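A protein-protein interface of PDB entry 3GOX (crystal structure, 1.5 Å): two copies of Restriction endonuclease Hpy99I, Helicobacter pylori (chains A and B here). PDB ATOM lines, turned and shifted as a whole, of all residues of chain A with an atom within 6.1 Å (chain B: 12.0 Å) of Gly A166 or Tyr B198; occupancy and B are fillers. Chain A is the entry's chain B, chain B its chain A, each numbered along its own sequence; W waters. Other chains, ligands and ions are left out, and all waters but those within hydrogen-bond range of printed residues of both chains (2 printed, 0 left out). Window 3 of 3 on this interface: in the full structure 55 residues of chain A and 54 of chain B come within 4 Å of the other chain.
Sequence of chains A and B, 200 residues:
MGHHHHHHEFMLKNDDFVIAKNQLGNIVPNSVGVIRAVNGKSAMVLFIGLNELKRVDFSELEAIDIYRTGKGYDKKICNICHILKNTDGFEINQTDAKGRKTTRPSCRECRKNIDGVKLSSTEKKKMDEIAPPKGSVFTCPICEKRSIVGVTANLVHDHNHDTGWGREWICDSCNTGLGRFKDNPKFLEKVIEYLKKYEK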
ATOM      1  N   LEU A 119       9.091  -0.152 -13.109  1.00  0.00           N
ATOM      2  CA  LEU A 119       9.899  -1.323 -13.419  1.00  0.00           C
ATOM      3  C   LEU A 119      11.227  -0.844 -13.988  1.00  0.00           C
ATOM      4  O   LEU A 119      11.260  -0.104 -14.980  1.00  0.00           O
ATOM      5  CB  LEU A 119       9.172  -2.229 -14.424  1.00  0.00           C
ATOM      6  CG  LEU A 119       9.889  -3.487 -14.924  1.00  0.00           C
ATOM      7  CD1 LEU A 119      10.169  -4.471 -13.800  1.00  0.00           C
ATOM      8  CD2 LEU A 119       9.067  -4.155 -16.020  1.00  0.00           C
ATOM      9  N   GLU A 123      15.416  -5.013 -14.803  1.00  0.00           N
ATOM     10  CA  GLU A 123      14.364  -5.967 -14.454  1.00  0.00           C
ATOM     11  C   GLU A 123      13.434  -6.212 -15.644  1.00  0.00           C
ATOM     12  O   GLU A 123      13.000  -7.336 -15.864  1.00  0.00           O
ATOM     13  CB  GLU A 123      13.575  -5.486 -13.238  1.00  0.00           C
ATOM     14  CG  GLU A 123      14.326  -5.590 -11.923  1.00  0.00           C
ATOM     15  CD  GLU A 123      14.495  -7.020 -11.444  1.00  0.00           C
ATOM     16  OE1 GLU A 123      15.656  -7.442 -11.249  1.00  0.00           O
ATOM     17  OE2 GLU A 123      13.487  -7.738 -11.278  1.00  0.00           O
ATOM     18  N   MET A 127      12.684  -9.813 -17.689  1.00  0.00           N
ATOM     19  CA  MET A 127      11.350 -10.315 -17.974  1.00  0.00           C
ATOM     20  C   MET A 127      11.188 -10.574 -19.469  1.00  0.00           C
ATOM     21  O   MET A 127      10.561 -11.559 -19.874  1.00  0.00           O
ATOM     22  CB  MET A 127      10.280  -9.353 -17.453  1.00  0.00           C
ATOM     23  CG  MET A 127      10.269  -9.265 -15.939  1.00  0.00           C
ATOM     24  SD  MET A 127       8.823  -8.426 -15.280  1.00  0.00           S
ATOM     25  CE  MET A 127       7.581  -9.696 -15.499  1.00  0.00           C
ATOM     26  N   ASP A 158       4.125  -7.545 -15.004  1.00  0.00           N
ATOM     27  CA  ASP A 158       3.800  -7.049 -13.665  1.00  0.00           C
ATOM     28  C   ASP A 158       5.075  -6.795 -12.856  1.00  0.00           C
ATOM     29  O   ASP A 158       6.096  -7.449 -13.048  1.00  0.00           O
ATOM     30  CB  ASP A 158       2.904  -8.081 -12.982  1.00  0.00           C
ATOM     31  CG  ASP A 158       2.494  -7.688 -11.604  1.00  0.00           C
ATOM     32  OD1 ASP A 158       2.236  -6.482 -11.355  1.00  0.00           O
ATOM     33  OD2 ASP A 158       2.403  -8.606 -10.762  1.00  0.00           O
ATOM     34  N   HIS A 159       5.023  -5.796 -11.979  1.00  0.00           N
ATOM     35  CA  HIS A 159       6.185  -5.444 -11.148  1.00  0.00           C
ATOM     36  C   HIS A 159       5.736  -4.932  -9.796  1.00  0.00           C
ATOM     37  O   HIS A 159       4.589  -4.490  -9.644  1.00  0.00           O
ATOM     38  CB  HIS A 159       7.089  -4.406 -11.839  1.00  0.00           C
ATOM     39  CG  HIS A 159       6.631  -2.985 -11.690  1.00  0.00           C
ATOM     40  ND1 HIS A 159       5.607  -2.452 -12.444  1.00  0.00           N
ATOM     41  CD2 HIS A 159       7.075  -1.982 -10.894  1.00  0.00           C
ATOM     42  CE1 HIS A 159       5.435  -1.182 -12.109  1.00  0.00           C
ATOM     43  NE2 HIS A 159       6.318  -0.872 -11.174  1.00  0.00           N
ATOM     44  N   ASN A 160       6.646  -5.006  -8.829  1.00  0.00           N
ATOM     45  CA  ASN A 160       6.406  -4.490  -7.493  1.00  0.00           C
ATOM     46  C   ASN A 160       6.765  -3.006  -7.492  1.00  0.00           C
ATOM     47  O   ASN A 160       7.897  -2.639  -7.807  1.00  0.00           O
ATOM     48  CB  ASN A 160       7.244  -5.270  -6.473  1.00  0.00           C
ATOM     49  CG  ASN A 160       7.015  -4.800  -5.056  1.00  0.00           C
ATOM     50  OD1 ASN A 160       7.305  -3.655  -4.730  1.00  0.00           O
ATOM     51  ND2 ASN A 160       6.488  -5.677  -4.209  1.00  0.00           N
ATOM     52  N   THR A 163       9.563  -1.625  -4.840  1.00  0.00           N
ATOM     53  CA  THR A 163      10.969  -1.936  -5.119  1.00  0.00           C
ATOM     54  C   THR A 163      11.412  -1.631  -6.554  1.00  0.00           C
ATOM     55  O   THR A 163      12.595  -1.375  -6.797  1.00  0.00           O
ATOM     56  CB  THR A 163      11.256  -3.433  -4.855  1.00  0.00           C
ATOM     57  OG1 THR A 163      10.453  -4.246  -5.733  1.00  0.00           O
ATOM     58  CG2 THR A 163      10.951  -3.786  -3.407  1.00  0.00           C
ATOM     59  N   GLY A 164      10.475  -1.695  -7.501  1.00  0.00           N
ATOM     60  CA  GLY A 164      10.788  -1.549  -8.926  1.00  0.00           C
ATOM     61  C   GLY A 164      11.232  -2.859  -9.573  1.00  0.00           C
ATOM     62  O   GLY A 164      11.663  -2.889 -10.730  1.00  0.00           O
ATOM     63  N   TRP A 165      11.116  -3.951  -8.824  1.00  0.00           N
ATOM     64  CA  TRP A 165      11.548  -5.255  -9.304  1.00  0.00           C
ATOM     65  C   TRP A 165      10.404  -5.998  -9.977  1.00  0.00           C
ATOM     66  O   TRP A 165       9.238  -5.823  -9.625  1.00  0.00           O
ATOM     67  CB  TRP A 165      12.128  -6.078  -8.152  1.00  0.00           C
ATOM     68  CG  TRP A 165      13.333  -5.425  -7.489  1.00  0.00           C
ATOM     69  CD1 TRP A 165      14.197  -4.524  -8.057  1.00  0.00           C
ATOM     70  CD2 TRP A 165      13.798  -5.629  -6.148  1.00  0.00           C
ATOM     71  NE1 TRP A 165      15.156  -4.149  -7.151  1.00  0.00           N
ATOM     72  CE2 TRP A 165      14.935  -4.809  -5.971  1.00  0.00           C
ATOM     73  CE3 TRP A 165      13.353  -6.409  -5.074  1.00  0.00           C
ATOM     74  CZ2 TRP A 165      15.646  -4.762  -4.766  1.00  0.00           C
ATOM     75  CZ3 TRP A 165      14.061  -6.360  -3.876  1.00  0.00           C
ATOM     76  CH2 TRP A 165      15.194  -5.540  -3.733  1.00  0.00           C
ATOM     77  N   GLY A 166      10.756  -6.832 -10.951  1.00  0.00           N
ATOM     78  CA  GLY A 166       9.778  -7.568 -11.715  1.00  0.00           C
ATOM     79  C   GLY A 166       9.103  -8.643 -10.889  1.00  0.00           C
ATOM     80  O   GLY A 166       9.691  -9.163  -9.931  1.00  0.00           O
ATOM     81  N   ARG A 167       7.854  -8.950 -11.243  1.00  0.00           N
ATOM     82  CA  ARG A 167       7.157 -10.115 -10.702  1.00  0.00           C
ATOM     83  C   ARG A 167       7.063 -11.153 -11.841  1.00  0.00           C
ATOM     84  O   ARG A 167       8.097 -11.703 -12.245  1.00  0.00           O
ATOM     85  CB  ARG A 167       5.816  -9.719 -10.053  1.00  0.00           C
ATOM     86  CG  ARG A 167       6.010  -8.825  -8.802  1.00  0.00           C
ATOM     87  CD  ARG A 167       4.819  -8.834  -7.848  1.00  0.00           C
ATOM     88  NE  ARG A 167       3.725  -8.012  -8.357  1.00  0.00           N
ATOM     89  CZ  ARG A 167       3.196  -6.943  -7.756  1.00  0.00           C
ATOM     90  NH1 ARG A 167       3.647  -6.526  -6.576  1.00  0.00           N
ATOM     91  NH2 ARG A 167       2.207  -6.271  -8.328  1.00  0.00           N
ATOM     92  N   GLU A 168       5.871 -11.408 -12.373  1.00  0.00           N
ATOM     93  CA  GLU A 168       5.692 -12.394 -13.443  1.00  0.00           C
ATOM     94  C   GLU A 168       4.839 -11.850 -14.583  1.00  0.00           C
ATOM     95  O   GLU A 168       4.189 -10.825 -14.449  1.00  0.00           O
ATOM     96  CB  GLU A 168       5.063 -13.692 -12.902  1.00  0.00           C
ATOM     97  CG  GLU A 168       5.879 -14.329 -11.791  1.00  0.00           C
ATOM     98  CD  GLU A 168       5.267 -15.584 -11.178  1.00  0.00           C
ATOM     99  OE1 GLU A 168       4.340 -16.184 -11.760  1.00  0.00           O
ATOM    100  OE2 GLU A 168       5.765 -15.996 -10.098  1.00  0.00           O
ATOM    101  N   GLU B 189      -6.537 -16.084  -2.653  1.00  0.00           N
ATOM    102  CA  GLU B 189      -5.441 -16.680  -1.894  1.00  0.00           C
ATOM    103  C   GLU B 189      -4.217 -16.822  -2.796  1.00  0.00           C
ATOM    104  O   GLU B 189      -3.093 -16.581  -2.374  1.00  0.00           O
ATOM    105  CB  GLU B 189      -5.852 -18.030  -1.308  1.00  0.00           C
ATOM    106  CG  GLU B 189      -6.867 -17.930  -0.161  1.00  0.00           C
ATOM    107  CD  GLU B 189      -6.262 -17.483   1.172  1.00  0.00           C
ATOM    108  OE1 GLU B 189      -5.091 -17.032   1.194  1.00  0.00           O
ATOM    109  OE2 GLU B 189      -6.964 -17.583   2.212  1.00  0.00           O
ATOM    110  N   LYS B 190      -4.455 -17.167  -4.052  1.00  0.00           N
ATOM    111  CA  LYS B 190      -3.376 -17.211  -5.034  1.00  0.00           C
ATOM    112  C   LYS B 190      -2.749 -15.828  -5.236  1.00  0.00           C
ATOM    113  O   LYS B 190      -1.529 -15.711  -5.336  1.00  0.00           O
ATOM    114  CB  LYS B 190      -3.877 -17.776  -6.352  1.00  0.00           C
ATOM    115  CG  LYS B 190      -4.120 -19.268  -6.279  1.00  0.00           C
ATOM    116  CD  LYS B 190      -4.146 -19.879  -7.630  1.00  0.00           C
ATOM    117  CE  LYS B 190      -2.747 -19.994  -8.210  1.00  0.00           C
ATOM    118  NZ  LYS B 190      -2.835 -20.161  -9.670  1.00  0.00           N
ATOM    119  N   VAL B 191      -3.576 -14.787  -5.271  1.00  0.00           N
ATOM    120  CA  VAL B 191      -3.054 -13.428  -5.378  1.00  0.00           C
ATOM    121  C   VAL B 191      -2.157 -13.082  -4.182  1.00  0.00           C
ATOM    122  O   VAL B 191      -1.086 -12.512  -4.346  1.00  0.00           O
ATOM    123  CB  VAL B 191      -4.171 -12.374  -5.456  1.00  0.00           C
ATOM    124  CG1 VAL B 191      -3.568 -10.981  -5.474  1.00  0.00           C
ATOM    125  CG2 VAL B 191      -5.067 -12.584  -6.689  1.00  0.00           C
ATOM    126  N   ILE B 192      -2.611 -13.426  -2.979  1.00  0.00           N
ATOM    127  CA  ILE B 192      -1.850 -13.143  -1.761  1.00  0.00           C
ATOM    128  C   ILE B 192      -0.469 -13.804  -1.783  1.00  0.00           C
ATOM    129  O   ILE B 192       0.546 -13.169  -1.490  1.00  0.00           O
ATOM    130  CB  ILE B 192      -2.633 -13.582  -0.497  1.00  0.00           C
ATOM    131  CG1 ILE B 192      -3.848 -12.670  -0.288  1.00  0.00           C
ATOM    132  CG2 ILE B 192      -1.734 -13.553   0.742  1.00  0.00           C
ATOM    133  CD1 ILE B 192      -4.747 -13.117   0.861  1.00  0.00           C
ATOM    134  N   GLU B 193      -0.421 -15.070  -2.163  1.00  0.00           N
ATOM    135  CA  GLU B 193       0.846 -15.787  -2.126  1.00  0.00           C
ATOM    136  C   GLU B 193       1.774 -15.296  -3.235  1.00  0.00           C
ATOM    137  O   GLU B 193       2.988 -15.249  -3.059  1.00  0.00           O
ATOM    138  CB  GLU B 193       0.595 -17.293  -2.200  1.00  0.00           C
ATOM    139  CG  GLU B 193      -0.197 -17.809  -0.983  1.00  0.00           C
ATOM    140  CD  GLU B 193       0.470 -17.490   0.370  1.00  0.00           C
ATOM    141  OE1 GLU B 193       1.647 -17.872   0.568  1.00  0.00           O
ATOM    142  OE2 GLU B 193      -0.182 -16.862   1.241  1.00  0.00           O
ATOM    143  N   TYR B 194       1.185 -14.898  -4.363  1.00  0.00           N
ATOM    144  CA  TYR B 194       1.932 -14.297  -5.470  1.00  0.00           C
ATOM    145  C   TYR B 194       2.587 -12.983  -5.030  1.00  0.00           C
ATOM    146  O   TYR B 194       3.774 -12.774  -5.268  1.00  0.00           O
ATOM    147  CB  TYR B 194       0.991 -14.080  -6.666  1.00  0.00           C
ATOM    148  CG  TYR B 194       1.554 -13.292  -7.836  1.00  0.00           C
ATOM    149  CD1 TYR B 194       2.205 -13.925  -8.875  1.00  0.00           C
ATOM    150  CD2 TYR B 194       1.372 -11.914  -7.934  1.00  0.00           C
ATOM    151  CE1 TYR B 194       2.701 -13.212  -9.960  1.00  0.00           C
ATOM    152  CE2 TYR B 194       1.865 -11.193  -9.028  1.00  0.00           C
ATOM    153  CZ  TYR B 194       2.530 -11.851 -10.040  1.00  0.00           C
ATOM    154  OH  TYR B 194       3.048 -11.192 -11.135  1.00  0.00           O
ATOM    155  N   LEU B 195       1.813 -12.113  -4.384  1.00  0.00           N
ATOM    156  CA  LEU B 195       2.328 -10.817  -3.916  1.00  0.00           C
ATOM    157  C   LEU B 195       3.401 -11.003  -2.843  1.00  0.00           C
ATOM    158  O   LEU B 195       4.492 -10.424  -2.930  1.00  0.00           O
ATOM    159  CB  LEU B 195       1.200  -9.939  -3.365  1.00  0.00           C
ATOM    160  CG  LEU B 195       0.137  -9.438  -4.347  1.00  0.00           C
ATOM    161  CD1 LEU B 195      -1.005  -8.735  -3.619  1.00  0.00           C
ATOM    162  CD2 LEU B 195       0.733  -8.523  -5.411  1.00  0.00           C
ATOM    163  N   LYS B 196       3.082 -11.831  -1.847  1.00  0.00           N
ATOM    164  CA  LYS B 196       3.990 -12.111  -0.733  1.00  0.00           C
ATOM    165  C   LYS B 196       5.326 -12.650  -1.226  1.00  0.00           C
ATOM    166  O   LYS B 196       6.383 -12.292  -0.705  1.00  0.00           O
ATOM    167  CB  LYS B 196       3.350 -13.095   0.254  1.00  0.00           C
ATOM    168  CG  LYS B 196       2.266 -12.472   1.149  1.00  0.00           C
ATOM    169  CD  LYS B 196       1.876 -13.400   2.305  1.00  0.00           C
ATOM    170  N   LYS B 197       5.261 -13.506  -2.242  1.00  0.00           N
ATOM    171  CA  LYS B 197       6.444 -14.065  -2.899  1.00  0.00           C
ATOM    172  C   LYS B 197       7.428 -13.002  -3.427  1.00  0.00           C
ATOM    173  O   LYS B 197       8.628 -13.237  -3.463  1.00  0.00           O
ATOM    174  CB  LYS B 197       6.006 -15.005  -4.036  1.00  0.00           C
ATOM    175  CG  LYS B 197       7.112 -15.453  -4.962  1.00  0.00           C
ATOM    176  CD  LYS B 197       6.688 -16.653  -5.788  1.00  0.00           C
ATOM    177  CE  LYS B 197       7.843 -17.185  -6.628  1.00  0.00           C
ATOM    178  NZ  LYS B 197       7.441 -18.390  -7.405  1.00  0.00           N
ATOM    179  N   TYR B 198       6.915 -11.848  -3.849  1.00  0.00           N
ATOM    180  CA  TYR B 198       7.756 -10.762  -4.376  1.00  0.00           C
ATOM    181  C   TYR B 198       7.776  -9.514  -3.481  1.00  0.00           C
ATOM    182  O   TYR B 198       8.202  -8.447  -3.934  1.00  0.00           O
ATOM    183  CB  TYR B 198       7.282 -10.375  -5.791  1.00  0.00           C
ATOM    184  CG  TYR B 198       7.424 -11.493  -6.789  1.00  0.00           C
ATOM    185  CD1 TYR B 198       8.673 -11.846  -7.273  1.00  0.00           C
ATOM    186  CD2 TYR B 198       6.316 -12.206  -7.237  1.00  0.00           C
ATOM    187  CE1 TYR B 198       8.823 -12.881  -8.176  1.00  0.00           C
ATOM    188  CE2 TYR B 198       6.458 -13.253  -8.143  1.00  0.00           C
ATOM    189  CZ  TYR B 198       7.714 -13.578  -8.615  1.00  0.00           C
ATOM    190  OH  TYR B 198       7.902 -14.610  -9.511  1.00  0.00           O
ATOM    191  N   GLU B 199       7.334  -9.653  -2.225  1.00  0.00           N
ATOM    192  CA  GLU B 199       7.250  -8.523  -1.286  1.00  0.00           C
ATOM    193  C   GLU B 199       8.543  -8.365  -0.489  1.00  0.00           C
ATOM    194  O   GLU B 199       9.620  -8.785  -0.929  1.00  0.00           O
ATOM    195  CB  GLU B 199       6.043  -8.685  -0.338  1.00  0.00           C
ATOM    196  CG  GLU B 199       5.634  -7.396   0.396  1.00  0.00           C
ATOM    197  CD  GLU B 199       4.134  -7.285   0.680  1.00  0.00           C
ATOM    198  OE1 GLU B 199       3.669  -7.884   1.678  1.00  0.00           O
ATOM    199  OE2 GLU B 199       3.427  -6.566  -0.078  1.00  0.00           O
HETATM  200  O   HOH W   1      10.131  -6.979  -5.273  1.00  0.00           O
HETATM  201  O   HOH W   2       4.524  -7.965  -4.142  1.00  0.00           O
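Gly A166 touches Tyr B198.
Arg A167 touches Tyr B194.
Arg A167 touches Leu B195.
Arg A167 touches Tyr B198.
No residue of chain B comes within 4 Å of Leu A119.
Of chain B, only Tyr B194 comes within 4 Å of Asp A158.
His A159 touches none of the printed residues of chain B.
Asn A160 touches just one residue of chain B: Tyr B198 (3.3 Å).
No residue of chain B comes within 4 Å of Thr A163.
Of chain B, only Tyr B198 comes within 4 Å of Gly A166.
Arg A167 touches just these residues of chain B: Tyr B194, Leu B195 and Tyr B198.
Printed residues of chain A within 4 Å of Tyr B194: Asp A158 (2.7 Å), Arg A167 (3.3 Å) and Glu A168 (3.1 Å).
Of the printed residues of chain A, Leu B195 touches Arg A167.
Printed residues of chain A within 4 Å of Lys B197: Glu A168 (3.97 Å).
Of chain A, only Asn A160 (3.3 Å), Gly A166 (3.9 Å), Arg A167 (3.6 Å) and Glu A168 (2.6 Å) come within 4 Å of Tyr B198.
The nearest residue of chain B that does not touch Gly A166 is Tyr B194 (6.6 Å).
The nearest printed residue of chain A that does not touch Tyr B194 is His A159 (5.8 Å).
Water W2 lies within hydrogen-bond range of O of Leu B195, NH1 of Arg A167 and ND2 of Asn A160.
Water W1 lies within hydrogen-bond range of the backbone carbonyl oxygen of Tyr B198 and the side-chain hydroxyl of Thr A163.
No position is printed for both chains.
OH of Tyr B194 lies within hydrogen-bond range of OD2 of Asp A158, at 2.7 Å.
The side-chain hydroxyl (OH) of Tyr B194 sits at hydrogen-bond distance from the backbone NH (N) of Glu A168, at 3.1 Å.
The side-chain amino group (NZ) of Lys B197 is in salt-bridge range of the side-chain carboxylate (OE2) of Glu A168 (3.97 Å).
The backbone carbonyl oxygen (O) of Tyr B198 sits at hydrogen-bond distance from the side-chain amide nitrogen (ND2) of Asn A160.
The side-chain hydroxyl of Tyr B198 lies within hydrogen-bond range of the side-chain carboxylate of Glu A168 (2.6 Å).
The backbone NH (N) of Gly A166 lies within hydrogen-bond range of the side-chain carboxylate (OE2) of Glu A123 (2.9 Å).
The guanidinium group (NE) of Arg A167 lies within salt-bridge range of the side-chain carboxylate (OD2) of Asp A158 (2.8 Å).
The backbone NH (N) of Asp A158 lies within hydrogen-bond range of the backbone carbonyl oxygen (O) of Glu A168.
The guanidinium group (NH2) of Arg A167 lies within hydrogen-bond range of the backbone carbonyl oxygen (O) of His A159.
OD1 of Asn A160 is in hydrogen-bond range of N of Thr A163.
N of Asn A160 sits at hydrogen-bond distance from O of Trp A165 (2.8 Å).
Of the 11 printed residues of chain B, 4 touch a printed residue of chain A.
Of the 12 printed residues of chain A, 5 touch a printed residue of chain B.
Among the printed residues, 9 pairs touch across the chains.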
